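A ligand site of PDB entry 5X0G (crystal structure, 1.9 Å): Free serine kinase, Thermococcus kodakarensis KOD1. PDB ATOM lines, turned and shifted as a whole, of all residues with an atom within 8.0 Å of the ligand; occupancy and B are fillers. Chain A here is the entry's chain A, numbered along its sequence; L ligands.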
ATOM      1  N   LYS A  15     -13.910  -2.691  29.628  1.00  0.00           N
ATOM      2  CA  LYS A  15     -13.193  -3.848  30.154  1.00  0.00           C
ATOM      3  C   LYS A  15     -13.710  -5.093  29.439  1.00  0.00           C
ATOM      4  O   LYS A  15     -14.635  -5.775  29.883  1.00  0.00           O
ATOM      5  CB  LYS A  15     -13.367  -3.915  31.671  1.00  0.00           C
ATOM      6  CG  LYS A  15     -12.429  -4.880  32.380  1.00  0.00           C
ATOM      7  CD  LYS A  15     -12.764  -5.030  33.860  1.00  0.00           C
ATOM      8  CE  LYS A  15     -12.441  -6.452  34.358  1.00  0.00           C
ATOM      9  N   VAL A  16     -13.090  -5.356  28.291  1.00  0.00           N
ATOM     10  CA  VAL A  16     -13.450  -6.516  27.467  1.00  0.00           C
ATOM     11  C   VAL A  16     -12.302  -7.500  27.608  1.00  0.00           C
ATOM     12  O   VAL A  16     -11.137  -7.116  27.453  1.00  0.00           O
ATOM     13  CB  VAL A  16     -13.729  -6.145  25.995  1.00  0.00           C
ATOM     14  CG1 VAL A  16     -15.022  -5.351  25.876  1.00  0.00           C
ATOM     15  CG2 VAL A  16     -12.589  -5.341  25.376  1.00  0.00           C
ATOM     16  N   ASP A  17     -12.613  -8.748  27.953  1.00  0.00           N
ATOM     17  CA  ASP A  17     -11.568  -9.754  28.147  1.00  0.00           C
ATOM     18  C   ASP A  17     -10.911 -10.074  26.798  1.00  0.00           C
ATOM     19  O   ASP A  17     -11.488  -9.848  25.742  1.00  0.00           O
ATOM     20  CB  ASP A  17     -12.132 -11.023  28.797  1.00  0.00           C
ATOM     21  CG  ASP A  17     -11.076 -11.858  29.498  1.00  0.00           C
ATOM     22  OD1 ASP A  17      -9.877 -11.475  29.540  1.00  0.00           O
ATOM     23  OD2 ASP A  17     -11.440 -12.945  29.993  1.00  0.00           O
ATOM     24  N   TYR A  18      -9.685 -10.588  26.865  1.00  0.00           N
ATOM     25  CA  TYR A  18      -8.971 -10.980  25.668  1.00  0.00           C
ATOM     26  C   TYR A  18      -9.017 -12.494  25.509  1.00  0.00           C
ATOM     27  O   TYR A  18      -9.282 -13.217  26.462  1.00  0.00           O
ATOM     28  CB  TYR A  18      -7.498 -10.507  25.720  1.00  0.00           C
ATOM     29  CG  TYR A  18      -6.709 -11.133  26.843  1.00  0.00           C
ATOM     30  CD1 TYR A  18      -6.063 -12.369  26.695  1.00  0.00           C
ATOM     31  CD2 TYR A  18      -6.637 -10.521  28.078  1.00  0.00           C
ATOM     32  CE1 TYR A  18      -5.354 -12.937  27.748  1.00  0.00           C
ATOM     33  CE2 TYR A  18      -5.944 -11.078  29.136  1.00  0.00           C
ATOM     34  CZ  TYR A  18      -5.312 -12.272  28.971  1.00  0.00           C
ATOM     35  OH  TYR A  18      -4.646 -12.774  30.058  1.00  0.00           O
ATOM     36  N   VAL A  19      -8.746 -12.942  24.293  1.00  0.00           N
ATOM     37  CA  VAL A  19      -8.536 -14.361  23.989  1.00  0.00           C
ATOM     38  C   VAL A  19      -7.228 -14.476  23.199  1.00  0.00           C
ATOM     39  O   VAL A  19      -6.916 -13.602  22.375  1.00  0.00           O
ATOM     40  CB  VAL A  19      -9.736 -14.935  23.191  1.00  0.00           C
ATOM     41  CG1 VAL A  19     -10.018 -14.130  21.922  1.00  0.00           C
ATOM     42  CG2 VAL A  19      -9.526 -16.411  22.900  1.00  0.00           C
ATOM     43  N   PHE A  20      -6.441 -15.519  23.472  1.00  0.00           N
ATOM     44  CA  PHE A  20      -5.217 -15.743  22.705  1.00  0.00           C
ATOM     45  C   PHE A  20      -5.589 -16.317  21.356  1.00  0.00           C
ATOM     46  O   PHE A  20      -6.330 -17.312  21.274  1.00  0.00           O
ATOM     47  CB  PHE A  20      -4.278 -16.711  23.424  1.00  0.00           C
ATOM     48  CG  PHE A  20      -3.596 -16.140  24.625  1.00  0.00           C
ATOM     49  CD1 PHE A  20      -2.681 -15.099  24.498  1.00  0.00           C
ATOM     50  CD2 PHE A  20      -3.844 -16.659  25.896  1.00  0.00           C
ATOM     51  CE1 PHE A  20      -2.043 -14.585  25.610  1.00  0.00           C
ATOM     52  CE2 PHE A  20      -3.221 -16.137  27.022  1.00  0.00           C
ATOM     53  CZ  PHE A  20      -2.306 -15.103  26.872  1.00  0.00           C
ATOM     54  N   ILE A  21      -5.077 -15.701  20.298  1.00  0.00           N
ATOM     55  CA  ILE A  21      -5.284 -16.129  18.931  1.00  0.00           C
ATOM     56  C   ILE A  21      -3.929 -16.298  18.300  1.00  0.00           C
ATOM     57  O   ILE A  21      -3.048 -15.477  18.505  1.00  0.00           O
ATOM     58  CB  ILE A  21      -6.112 -15.096  18.131  1.00  0.00           C
ATOM     59  CG1 ILE A  21      -7.502 -14.874  18.772  1.00  0.00           C
ATOM     60  CG2 ILE A  21      -6.253 -15.498  16.663  1.00  0.00           C
ATOM     61  CD1 ILE A  21      -8.410 -16.056  18.716  1.00  0.00           C
ATOM     62  N   ARG A  84       1.335 -16.396  19.393  1.00  0.00           N
ATOM     63  CA  ARG A  84      -0.013 -15.878  19.589  1.00  0.00           C
ATOM     64  C   ARG A  84       0.005 -14.458  20.131  1.00  0.00           C
ATOM     65  O   ARG A  84       1.057 -13.968  20.564  1.00  0.00           O
ATOM     66  CB  ARG A  84      -0.783 -16.774  20.553  1.00  0.00           C
ATOM     67  CG  ARG A  84      -0.231 -16.840  21.979  1.00  0.00           C
ATOM     68  CD  ARG A  84      -0.712 -18.068  22.721  1.00  0.00           C
ATOM     69  NE  ARG A  84      -0.053 -19.259  22.218  1.00  0.00           N
ATOM     70  CZ  ARG A  84       1.150 -19.706  22.592  1.00  0.00           C
ATOM     71  NH1 ARG A  84       1.859 -19.066  23.508  1.00  0.00           N
ATOM     72  NH2 ARG A  84       1.646 -20.806  22.045  1.00  0.00           N
ATOM     73  N   ALA A  85      -1.161 -13.840  20.136  1.00  0.00           N
ATOM     74  CA  ALA A  85      -1.355 -12.533  20.761  1.00  0.00           C
ATOM     75  C   ALA A  85      -2.705 -12.438  21.463  1.00  0.00           C
ATOM     76  O   ALA A  85      -3.708 -12.990  20.963  1.00  0.00           O
ATOM     77  CB  ALA A  85      -1.212 -11.440  19.735  1.00  0.00           C
ATOM     78  N   PRO A  86      -2.761 -11.744  22.628  1.00  0.00           N
ATOM     79  CA  PRO A  86      -4.078 -11.543  23.225  1.00  0.00           C
ATOM     80  C   PRO A  86      -4.842 -10.581  22.345  1.00  0.00           C
ATOM     81  O   PRO A  86      -4.276  -9.554  21.901  1.00  0.00           O
ATOM     82  CB  PRO A  86      -3.794 -10.943  24.600  1.00  0.00           C
ATOM     83  CG  PRO A  86      -2.358 -10.576  24.620  1.00  0.00           C
ATOM     84  CD  PRO A  86      -1.678 -11.151  23.419  1.00  0.00           C
ATOM     85  N   SER A  87      -6.108 -10.924  22.110  1.00  0.00           N
ATOM     86  CA  SER A  87      -6.906 -10.269  21.102  1.00  0.00           C
ATOM     87  C   SER A  87      -8.307 -10.044  21.618  1.00  0.00           C
ATOM     88  O   SER A  87      -8.805 -10.805  22.438  1.00  0.00           O
ATOM     89  CB  SER A  87      -6.995 -11.172  19.879  1.00  0.00           C
ATOM     90  OG  SER A  87      -5.715 -11.461  19.330  1.00  0.00           O
ATOM     91  N   ILE A 234      -4.343  -4.687  29.510  1.00  0.00           N
ATOM     92  CA  ILE A 234      -4.297  -6.069  30.008  1.00  0.00           C
ATOM     93  C   ILE A 234      -2.942  -6.430  30.589  1.00  0.00           C
ATOM     94  O   ILE A 234      -1.962  -5.757  30.307  1.00  0.00           O
ATOM     95  CB  ILE A 234      -4.696  -7.085  28.918  1.00  0.00           C
ATOM     96  CG1 ILE A 234      -3.784  -6.987  27.697  1.00  0.00           C
ATOM     97  CG2 ILE A 234      -6.130  -6.845  28.493  1.00  0.00           C
ATOM     98  CD1 ILE A 234      -3.977  -8.138  26.728  1.00  0.00           C
ATOM     99  N   ASP A 235      -2.914  -7.516  31.363  1.00  0.00           N
ATOM    100  CA  ASP A 235      -1.741  -7.989  32.078  1.00  0.00           C
ATOM    101  C   ASP A 235      -1.337  -9.325  31.461  1.00  0.00           C
ATOM    102  O   ASP A 235      -1.806 -10.387  31.888  1.00  0.00           O
ATOM    103  CB  ASP A 235      -2.106  -8.129  33.564  1.00  0.00           C
ATOM    104  CG  ASP A 235      -1.024  -8.807  34.387  1.00  0.00           C
ATOM    105  OD1 ASP A 235       0.171  -8.689  34.049  1.00  0.00           O
ATOM    106  OD2 ASP A 235      -1.379  -9.437  35.408  1.00  0.00           O
ATOM    107  N   VAL A 236      -0.502  -9.253  30.427  1.00  0.00           N
ATOM    108  CA  VAL A 236       0.030 -10.439  29.745  1.00  0.00           C
ATOM    109  C   VAL A 236       1.530 -10.258  29.627  1.00  0.00           C
ATOM    110  O   VAL A 236       2.006  -9.183  29.278  1.00  0.00           O
ATOM    111  CB  VAL A 236      -0.634 -10.646  28.354  1.00  0.00           C
ATOM    112  CG1 VAL A 236       0.055 -11.742  27.553  1.00  0.00           C
ATOM    113  CG2 VAL A 236      -2.104 -10.932  28.531  1.00  0.00           C
ATOM    114  N   GLU A 240       4.337 -15.484  27.685  1.00  0.00           N
ATOM    115  CA  GLU A 240       3.099 -16.214  27.387  1.00  0.00           C
ATOM    116  C   GLU A 240       2.780 -16.357  25.888  1.00  0.00           C
ATOM    117  O   GLU A 240       1.857 -17.104  25.531  1.00  0.00           O
ATOM    118  CB  GLU A 240       1.914 -15.542  28.085  1.00  0.00           C
ATOM    119  CG  GLU A 240       2.021 -15.468  29.597  1.00  0.00           C
ATOM    120  CD  GLU A 240       0.812 -14.781  30.217  1.00  0.00           C
ATOM    121  OE1 GLU A 240      -0.298 -15.315  30.078  1.00  0.00           O
ATOM    122  OE2 GLU A 240       0.965 -13.720  30.854  1.00  0.00           O
HETATM  123  O1  LIG L   1      -9.276 -17.482  26.591  1.00  0.00           O
HETATM  124  S1  LIG L   1      -7.864 -17.369  26.847  1.00  0.00           S
HETATM  125  O2  LIG L   1      -7.451 -18.504  27.622  1.00  0.00           O
HETATM  126  O3  LIG L   1      -7.095 -17.308  25.414  1.00  0.00           O
HETATM  127  C1  LIG L   1      -7.499 -15.980  27.681  1.00  0.00           C
HETATM  128  C2  LIG L   1      -8.477 -15.711  28.814  1.00  0.00           C
HETATM  129  O4  LIG L   1      -9.637 -15.081  28.265  1.00  0.00           O
HETATM  130  C3  LIG L   1      -7.844 -14.796  29.866  1.00  0.00           C
HETATM  131  N1  LIG L   1      -8.812 -14.244  30.848  1.00  0.00           N
HETATM  132  C4  LIG L   1      -9.291 -15.297  31.762  1.00  0.00           C
HETATM  133  C5  LIG L   1     -10.300 -14.713  32.746  1.00  0.00           C
HETATM  134  N2  LIG L   1      -9.713 -13.611  33.536  1.00  0.00           N
HETATM  135  C6  LIG L   1      -9.116 -12.575  32.671  1.00  0.00           C
HETATM  136  C7  LIG L   1      -8.155 -13.187  31.639  1.00  0.00           C
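N of Phe 20 is in hydrogen-bond range of O3 of the ligand, at 2.7 Å. O of Tyr 18 lies within hydrogen-bond range of O4 of the ligand, at 2.6 Å. A nitrogen (N1) of the ligand is in salt-bridge range of the side-chain carboxylate (OD2) of Asp 17 (3.1 Å).
The backbone carbonyl oxygen (O) of Val 19 is in hydrogen-bond range of the backbone NH (N) of Ser 87, 2.8 Å away.
Merely in contact with the ligand: Val 19. Hydrophobic or aromatic side chains within 4 Å of the ligand: Tyr 18, Val 19 and Phe 20. Four residues have an atom within 4 Å of the ligand: Asp 17, Tyr 18, Val 19 and Phe 20.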
